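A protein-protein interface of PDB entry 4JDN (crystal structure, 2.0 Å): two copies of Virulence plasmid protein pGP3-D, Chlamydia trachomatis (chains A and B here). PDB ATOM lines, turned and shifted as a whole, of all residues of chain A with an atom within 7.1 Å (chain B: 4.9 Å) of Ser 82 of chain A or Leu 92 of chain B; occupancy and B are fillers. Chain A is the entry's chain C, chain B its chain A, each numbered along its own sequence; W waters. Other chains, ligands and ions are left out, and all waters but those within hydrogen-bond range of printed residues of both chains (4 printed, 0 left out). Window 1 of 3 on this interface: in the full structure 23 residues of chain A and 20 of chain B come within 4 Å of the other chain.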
ATOM      1  N   ALA A  55     -12.152 -31.935  13.231  1.00  0.00           N
ATOM      2  CA  ALA A  55     -11.377 -30.889  13.869  1.00  0.00           C
ATOM      3  C   ALA A  55     -11.903 -29.569  13.332  1.00  0.00           C
ATOM      4  O   ALA A  55     -11.936 -29.362  12.122  1.00  0.00           O
ATOM      5  CB  ALA A  55      -9.894 -31.039  13.557  1.00  0.00           C
ATOM      6  N   ASP A  56     -12.322 -28.689  14.230  1.00  0.00           N
ATOM      7  CA  ASP A  56     -12.847 -27.391  13.841  1.00  0.00           C
ATOM      8  C   ASP A  56     -12.095 -26.315  14.613  1.00  0.00           C
ATOM      9  O   ASP A  56     -12.313 -26.098  15.803  1.00  0.00           O
ATOM     10  CB  ASP A  56     -14.360 -27.339  14.046  1.00  0.00           C
ATOM     11  CG  ASP A  56     -15.091 -28.377  13.177  1.00  0.00           C
ATOM     12  OD1 ASP A  56     -15.158 -28.201  11.940  1.00  0.00           O
ATOM     13  OD2 ASP A  56     -15.563 -29.385  13.726  1.00  0.00           O
ATOM     14  N   VAL A  66      -4.286 -22.200   5.183  1.00  0.00           N
ATOM     15  CA  VAL A  66      -4.009 -22.913   6.422  1.00  0.00           C
ATOM     16  C   VAL A  66      -4.051 -24.413   6.111  1.00  0.00           C
ATOM     17  O   VAL A  66      -4.943 -24.869   5.409  1.00  0.00           O
ATOM     18  CB  VAL A  66      -5.103 -22.611   7.473  1.00  0.00           C
ATOM     19  CG1 VAL A  66      -4.866 -23.398   8.740  1.00  0.00           C
ATOM     20  CG2 VAL A  66      -5.165 -21.115   7.771  1.00  0.00           C
ATOM     21  N   VAL A  67      -3.094 -25.172   6.627  1.00  0.00           N
ATOM     22  CA  VAL A  67      -3.091 -26.613   6.463  1.00  0.00           C
ATOM     23  C   VAL A  67      -3.271 -27.288   7.825  1.00  0.00           C
ATOM     24  O   VAL A  67      -2.708 -26.846   8.823  1.00  0.00           O
ATOM     25  CB  VAL A  67      -1.785 -27.091   5.794  1.00  0.00           C
ATOM     26  CG1 VAL A  67      -1.793 -28.607   5.604  1.00  0.00           C
ATOM     27  CG2 VAL A  67      -1.584 -26.383   4.457  1.00  0.00           C
ATOM     28  N   LEU A  68      -4.083 -28.344   7.866  1.00  0.00           N
ATOM     29  CA  LEU A  68      -4.271 -29.139   9.080  1.00  0.00           C
ATOM     30  C   LEU A  68      -3.845 -30.568   8.776  1.00  0.00           C
ATOM     31  O   LEU A  68      -4.205 -31.110   7.729  1.00  0.00           O
ATOM     32  CB  LEU A  68      -5.739 -29.155   9.531  1.00  0.00           C
ATOM     33  CG  LEU A  68      -6.398 -27.817   9.898  1.00  0.00           C
ATOM     34  CD1 LEU A  68      -6.848 -27.123   8.630  1.00  0.00           C
ATOM     35  CD2 LEU A  68      -7.600 -28.035  10.836  1.00  0.00           C
ATOM     36  N   ALA A  69      -3.103 -31.183   9.692  1.00  0.00           N
ATOM     37  CA  ALA A  69      -2.658 -32.564   9.483  1.00  0.00           C
ATOM     38  C   ALA A  69      -2.852 -33.395  10.741  1.00  0.00           C
ATOM     39  O   ALA A  69      -2.426 -33.001  11.822  1.00  0.00           O
ATOM     40  CB  ALA A  69      -1.211 -32.600   9.021  1.00  0.00           C
ATOM     41  N   LEU A  70      -3.528 -34.531  10.599  1.00  0.00           N
ATOM     42  CA  LEU A  70      -3.762 -35.425  11.726  1.00  0.00           C
ATOM     43  C   LEU A  70      -2.778 -36.578  11.622  1.00  0.00           C
ATOM     44  O   LEU A  70      -2.686 -37.204  10.573  1.00  0.00           O
ATOM     45  CB  LEU A  70      -5.183 -35.975  11.693  1.00  0.00           C
ATOM     46  CG  LEU A  70      -5.616 -36.876  12.850  1.00  0.00           C
ATOM     47  CD1 LEU A  70      -5.763 -36.080  14.164  1.00  0.00           C
ATOM     48  CD2 LEU A  70      -6.907 -37.560  12.489  1.00  0.00           C
ATOM     49  N   ALA A  80      -4.498 -37.946   7.612  1.00  0.00           N
ATOM     50  CA  ALA A  80      -5.502 -37.062   7.012  1.00  0.00           C
ATOM     51  C   ALA A  80      -4.980 -35.634   6.944  1.00  0.00           C
ATOM     52  O   ALA A  80      -4.306 -35.160   7.858  1.00  0.00           O
ATOM     53  CB  ALA A  80      -6.804 -37.117   7.796  1.00  0.00           C
ATOM     54  N   ILE A  81      -5.276 -34.963   5.842  1.00  0.00           N
ATOM     55  CA  ILE A  81      -4.815 -33.615   5.608  1.00  0.00           C
ATOM     56  C   ILE A  81      -5.991 -32.782   5.085  1.00  0.00           C
ATOM     57  O   ILE A  81      -6.735 -33.220   4.206  1.00  0.00           O
ATOM     58  CB  ILE A  81      -3.664 -33.601   4.585  1.00  0.00           C
ATOM     59  CG1 ILE A  81      -2.437 -34.312   5.173  1.00  0.00           C
ATOM     60  CG2 ILE A  81      -3.314 -32.175   4.185  1.00  0.00           C
ATOM     61  CD1 ILE A  81      -1.401 -34.723   4.136  1.00  0.00           C
ATOM     62  N   SER A  82      -6.179 -31.592   5.636  1.00  0.00           N
ATOM     63  CA  SER A  82      -7.242 -30.727   5.135  1.00  0.00           C
ATOM     64  C   SER A  82      -6.730 -29.291   5.019  1.00  0.00           C
ATOM     65  O   SER A  82      -5.576 -29.003   5.384  1.00  0.00           O
ATOM     66  CB  SER A  82      -8.485 -30.815   6.039  1.00  0.00           C
ATOM     67  OG  SER A  82      -9.592 -30.106   5.487  1.00  0.00           O
ATOM     68  N   TYR A  83      -7.587 -28.400   4.517  1.00  0.00           N
ATOM     69  CA  TYR A  83      -7.177 -27.043   4.144  1.00  0.00           C
ATOM     70  C   TYR A  83      -8.208 -26.021   4.582  1.00  0.00           C
ATOM     71  O   TYR A  83      -9.413 -26.266   4.500  1.00  0.00           O
ATOM     72  CB  TYR A  83      -6.973 -26.953   2.625  1.00  0.00           C
ATOM     73  CG  TYR A  83      -5.908 -27.917   2.159  1.00  0.00           C
ATOM     74  CD1 TYR A  83      -4.558 -27.562   2.201  1.00  0.00           C
ATOM     75  CD2 TYR A  83      -6.245 -29.198   1.739  1.00  0.00           C
ATOM     76  CE1 TYR A  83      -3.567 -28.462   1.824  1.00  0.00           C
ATOM     77  CE2 TYR A  83      -5.272 -30.107   1.362  1.00  0.00           C
ATOM     78  CZ  TYR A  83      -3.928 -29.727   1.396  1.00  0.00           C
ATOM     79  OH  TYR A  83      -2.955 -30.626   1.011  1.00  0.00           O
ATOM     80  N   GLY A  84      -7.724 -24.884   5.067  1.00  0.00           N
ATOM     81  CA  GLY A  84      -8.583 -23.767   5.393  1.00  0.00           C
ATOM     82  C   GLY A  84      -8.019 -22.472   4.839  1.00  0.00           C
ATOM     83  O   GLY A  84      -7.000 -22.466   4.131  1.00  0.00           O
ATOM     84  N   TYR A  85      -8.659 -21.364   5.194  1.00  0.00           N
ATOM     85  CA  TYR A  85      -8.307 -20.075   4.629  1.00  0.00           C
ATOM     86  C   TYR A  85      -8.561 -18.949   5.614  1.00  0.00           C
ATOM     87  O   TYR A  85      -9.553 -18.958   6.338  1.00  0.00           O
ATOM     88  CB  TYR A  85      -9.134 -19.816   3.368  1.00  0.00           C
ATOM     89  CG  TYR A  85      -9.035 -18.385   2.852  1.00  0.00           C
ATOM     90  CD1 TYR A  85      -7.891 -17.940   2.179  1.00  0.00           C
ATOM     91  CD2 TYR A  85     -10.087 -17.485   3.031  1.00  0.00           C
ATOM     92  CE1 TYR A  85      -7.796 -16.622   1.710  1.00  0.00           C
ATOM     93  CE2 TYR A  85     -10.008 -16.162   2.558  1.00  0.00           C
ATOM     94  CZ  TYR A  85      -8.867 -15.744   1.900  1.00  0.00           C
ATOM     95  OH  TYR A  85      -8.790 -14.452   1.434  1.00  0.00           O
ATOM     96  N   LEU A  92     -13.049 -20.390  10.631  1.00  0.00           N
ATOM     97  CA  LEU A  92     -13.014 -21.791  11.031  1.00  0.00           C
ATOM     98  C   LEU A  92     -12.310 -22.600   9.963  1.00  0.00           C
ATOM     99  O   LEU A  92     -12.693 -22.569   8.783  1.00  0.00           O
ATOM    100  CB  LEU A  92     -14.421 -22.354  11.258  1.00  0.00           C
ATOM    101  CG  LEU A  92     -14.486 -23.618  12.129  1.00  0.00           C
ATOM    102  CD1 LEU A  92     -13.981 -23.345  13.555  1.00  0.00           C
ATOM    103  CD2 LEU A  92     -15.915 -24.156  12.147  1.00  0.00           C
ATOM    104  N   CYS A  93     -11.276 -23.319  10.382  1.00  0.00           N
ATOM    105  CA  CYS A  93     -10.517 -24.197   9.492  1.00  0.00           C
ATOM    106  C   CYS A  93     -10.733 -25.628   9.956  1.00  0.00           C
ATOM    107  O   CYS A  93     -10.538 -25.941  11.143  1.00  0.00           O
ATOM    108  CB  CYS A  93      -9.035 -23.837   9.538  1.00  0.00           C
ATOM    109  SG  CYS A  93      -8.702 -22.140   8.982  1.00  0.00           S
ATOM    110  N   SER A  94     -11.142 -26.491   9.029  1.00  0.00           N
ATOM    111  CA  SER A  94     -11.687 -27.789   9.411  1.00  0.00           C
ATOM    112  C   SER A  94     -11.018 -28.974   8.750  1.00  0.00           C
ATOM    113  O   SER A  94     -10.503 -28.878   7.627  1.00  0.00           O
ATOM    114  CB  SER A  94     -13.194 -27.827   9.121  1.00  0.00           C
ATOM    115  OG  SER A  94     -13.890 -27.008  10.044  1.00  0.00           O
ATOM    116  N   LEU A  95     -11.037 -30.095   9.467  1.00  0.00           N
ATOM    117  CA  LEU A  95     -10.615 -31.385   8.938  1.00  0.00           C
ATOM    118  C   LEU A  95     -11.694 -32.412   9.260  1.00  0.00           C
ATOM    119  O   LEU A  95     -12.174 -32.483  10.393  1.00  0.00           O
ATOM    120  CB  LEU A  95      -9.286 -31.819   9.568  1.00  0.00           C
ATOM    121  CG  LEU A  95      -8.679 -33.160   9.131  1.00  0.00           C
ATOM    122  CD1 LEU A  95      -7.143 -33.059   9.108  1.00  0.00           C
ATOM    123  CD2 LEU A  95      -9.107 -34.285  10.062  1.00  0.00           C
ATOM    124  N   ARG A  96     -12.078 -33.190   8.257  1.00  0.00           N
ATOM    125  CA  ARG A  96     -13.013 -34.286   8.435  1.00  0.00           C
ATOM    126  C   ARG A  96     -12.369 -35.551   7.893  1.00  0.00           C
ATOM    127  O   ARG A  96     -11.756 -35.532   6.827  1.00  0.00           O
ATOM    128  CB  ARG A  96     -14.286 -34.040   7.637  1.00  0.00           C
ATOM    129  CG  ARG A  96     -15.094 -32.890   8.129  1.00  0.00           C
ATOM    130  CD  ARG A  96     -15.819 -33.260   9.414  1.00  0.00           C
ATOM    131  NE  ARG A  96     -16.645 -32.142   9.847  1.00  0.00           N
ATOM    132  CZ  ARG A  96     -16.166 -31.074  10.480  1.00  0.00           C
ATOM    133  NH1 ARG A  96     -14.871 -31.005  10.773  1.00  0.00           N
ATOM    134  NH2 ARG A  96     -16.981 -30.087  10.835  1.00  0.00           N
ATOM    135  N   ASP B  56     -17.565 -32.640   2.659  1.00  0.00           N
ATOM    136  CA  ASP B  56     -16.482 -31.713   2.943  1.00  0.00           C
ATOM    137  C   ASP B  56     -15.433 -31.819   1.850  1.00  0.00           C
ATOM    138  O   ASP B  56     -14.641 -32.758   1.811  1.00  0.00           O
ATOM    139  CB  ASP B  56     -15.921 -31.973   4.341  1.00  0.00           C
ATOM    140  CG  ASP B  56     -16.971 -31.741   5.416  1.00  0.00           C
ATOM    141  OD1 ASP B  56     -17.264 -30.565   5.727  1.00  0.00           O
ATOM    142  OD2 ASP B  56     -17.540 -32.727   5.917  1.00  0.00           O
ATOM    143  N   ILE B  57     -15.462 -30.838   0.950  1.00  0.00           N
ATOM    144  CA  ILE B  57     -14.764 -30.927  -0.320  1.00  0.00           C
ATOM    145  C   ILE B  57     -13.643 -29.889  -0.442  1.00  0.00           C
ATOM    146  O   ILE B  57     -13.888 -28.676  -0.357  1.00  0.00           O
ATOM    147  CB  ILE B  57     -15.766 -30.706  -1.480  1.00  0.00           C
ATOM    148  CG1 ILE B  57     -17.015 -31.602  -1.304  1.00  0.00           C
ATOM    149  CG2 ILE B  57     -15.083 -30.930  -2.833  1.00  0.00           C
ATOM    150  CD1 ILE B  57     -16.704 -33.101  -1.276  1.00  0.00           C
ATOM    151  N   ILE B  58     -12.420 -30.370  -0.646  1.00  0.00           N
ATOM    152  CA  ILE B  58     -11.279 -29.495  -0.897  1.00  0.00           C
ATOM    153  C   ILE B  58     -11.400 -28.938  -2.317  1.00  0.00           C
ATOM    154  O   ILE B  58     -11.510 -29.703  -3.270  1.00  0.00           O
ATOM    155  CB  ILE B  58      -9.944 -30.277  -0.757  1.00  0.00           C
ATOM    156  CG1 ILE B  58      -9.792 -30.848   0.656  1.00  0.00           C
ATOM    157  CG2 ILE B  58      -8.755 -29.394  -1.099  1.00  0.00           C
ATOM    158  CD1 ILE B  58      -8.679 -31.874   0.777  1.00  0.00           C
ATOM    159  N   PRO B  90      -6.493 -23.543  -1.972  1.00  0.00           N
ATOM    160  CA  PRO B  90      -7.482 -24.567  -1.602  1.00  0.00           C
ATOM    161  C   PRO B  90      -8.161 -24.218  -0.286  1.00  0.00           C
ATOM    162  O   PRO B  90      -7.517 -23.685   0.626  1.00  0.00           O
ATOM    163  CB  PRO B  90      -6.634 -25.827  -1.411  1.00  0.00           C
ATOM    164  CG  PRO B  90      -5.367 -25.570  -2.159  1.00  0.00           C
ATOM    165  CD  PRO B  90      -5.129 -24.097  -2.067  1.00  0.00           C
ATOM    166  N   ASN B  91      -9.449 -24.535  -0.200  1.00  0.00           N
ATOM    167  CA  ASN B  91     -10.230 -24.321   1.011  1.00  0.00           C
ATOM    168  C   ASN B  91     -11.290 -25.407   1.077  1.00  0.00           C
ATOM    169  O   ASN B  91     -11.718 -25.931   0.040  1.00  0.00           O
ATOM    170  CB  ASN B  91     -10.877 -22.927   0.977  1.00  0.00           C
ATOM    171  CG  ASN B  91     -11.516 -22.539   2.301  1.00  0.00           C
ATOM    172  OD1 ASN B  91     -11.126 -23.040   3.350  1.00  0.00           O
ATOM    173  ND2 ASN B  91     -12.507 -21.647   2.253  1.00  0.00           N
ATOM    174  N   LEU B  92     -11.703 -25.770   2.285  1.00  0.00           N
ATOM    175  CA  LEU B  92     -12.744 -26.767   2.449  1.00  0.00           C
ATOM    176  C   LEU B  92     -14.096 -26.118   2.134  1.00  0.00           C
ATOM    177  O   LEU B  92     -14.440 -25.049   2.645  1.00  0.00           O
ATOM    178  CB  LEU B  92     -12.727 -27.365   3.869  1.00  0.00           C
ATOM    179  CG  LEU B  92     -13.440 -28.719   4.055  1.00  0.00           C
ATOM    180  CD1 LEU B  92     -12.810 -29.826   3.169  1.00  0.00           C
ATOM    181  CD2 LEU B  92     -13.492 -29.157   5.541  1.00  0.00           C
ATOM    182  N   CYS B  93     -14.841 -26.758   1.249  1.00  0.00           N
ATOM    183  CA  CYS B  93     -16.146 -26.272   0.855  1.00  0.00           C
ATOM    184  C   CYS B  93     -17.144 -27.348   1.273  1.00  0.00           C
ATOM    185  O   CYS B  93     -16.999 -28.514   0.898  1.00  0.00           O
ATOM    186  CB  CYS B  93     -16.181 -26.052  -0.651  1.00  0.00           C
ATOM    187  SG  CYS B  93     -15.092 -24.705  -1.243  1.00  0.00           S
ATOM    188  N   SER B  94     -18.145 -26.960   2.053  1.00  0.00           N
ATOM    189  CA  SER B  94     -18.982 -27.943   2.738  1.00  0.00           C
ATOM    190  C   SER B  94     -20.478 -27.803   2.496  1.00  0.00           C
ATOM    191  O   SER B  94     -20.997 -26.699   2.304  1.00  0.00           O
ATOM    192  CB  SER B  94     -18.730 -27.891   4.249  1.00  0.00           C
ATOM    193  OG  SER B  94     -17.355 -28.077   4.544  1.00  0.00           O
HETATM  194  O   HOH W   1     -13.077 -34.040   4.019  1.00  0.00           O
HETATM  195  O   HOH W   2      -5.094 -23.799   2.017  1.00  0.00           O
HETATM  196  O   HOH W   3     -19.089 -32.620   8.942  1.00  0.00           O
HETATM  197  O   HOH W   4     -11.310 -22.116   6.134  1.00  0.00           O
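The backbone NH (N) of Leu 92 of chain B sits at hydrogen-bond distance from the backbone carbonyl oxygen (O) of Tyr 83 of chain A (3.2 Å).
OD1 of Asp 56 of chain B is in hydrogen-bond range of OG of Ser 94 of chain B (2.8 Å). OD1 of Asp 56 of chain A lies within hydrogen-bond range of OG of Ser 94 of chain A, 2.6 Å away. The side-chain carboxylate of Asp 56 of chain A lies within salt-bridge range of the guanidinium group of Arg 96 of chain A (2.8 Å). O of Val 66 of chain A sits at hydrogen-bond distance from N of Gly 84 of chain A (2.8 Å). The backbone carbonyl oxygen of Leu 68 of chain A sits at hydrogen-bond distance from the backbone NH of Ser 82 of chain A, at 2.9 Å. OG of Ser 82 of chain A is in hydrogen-bond range of O of Ser 94 of chain A, at 2.6 Å.
Among the printed residues, pairs that only touch across the chains: Ser 82 of chain A with Leu 92 of chain B, Tyr 83 of chain A with Ile 58 of chain B, Tyr 83 of chain A with Pro 90 of chain B, Tyr 83 of chain A with Asn 91 of chain B, Gly 84 of chain A with Pro 90 of chain B, Gly 84 of chain A with Asn 91 of chain B, Tyr 85 of chain A with Asn 91 of chain B, Ser 94 of chain A with Leu 92 of chain B and Arg 96 of chain A with Asp 56 of chain B.
Ser 82 of chain A touches just one residue of chain B: Leu 92 (3.98 Å). Leu 92 of chain B touches just these residues of chain A: Ser 82 (3.98 Å), Tyr 83 (3.2 Å) and Ser 94 (3.7 Å). Printed residues of chain A within 4 Å of Ile 58 of chain B: Tyr 83. Of the printed residues of chain B, Tyr 85 of chain A touches Asn 91 (3.5 Å). Leu 68 of chain A touches none of the printed residues of chain B. Cys 93 of chain A touches none of the printed residues of chain B. The nearest residue of chain B that does not touch Ser 82 of chain A is Ile 58 of chain B (4.7 Å).
Printed residues of chain B that touch a printed residue of chain A: Asp 56, Ile 58, Pro 90, Asn 91 and Leu 92. Hydrophobic or aromatic side chains of chain B within 4 Å of the printed part of chain A: Ile 58 and Leu 92. Among the printed residues, no Asp or Glu carboxylate lies within 4 Å of a Lys or Arg side-chain nitrogen of the other chain.
Ser 94 of chain A touches Leu 92 of chain B, but with the chains exchanged Leu 92 of chain A does not touch Ser 94 of chain B (8.4 Å). Of the 10 pairs that touch across the chains among the printed residues, none has its exchanged pair printed and touching as well.
Water W3 lies within hydrogen-bond range of NE of Arg 96 of chain A (2.6 Å) and OD2 of Asp 56 of chain B (3.4 Å). Water W2 bridges O of Pro 90 of chain B (2.8 Å) and O of Gly 84 of chain A (3.1 Å). Water W4 lies within hydrogen-bond range of the backbone NH of Tyr 85 of chain A, the side-chain amide oxygen of Asn 91 of chain B and the backbone carbonyl oxygen of Leu 92 of chain A. Water W1 bridges the backbone carbonyl oxygen of Asp 56 of chain B (3.0 Å) and the backbone carbonyl oxygen of Arg 96 of chain A (3.4 Å).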
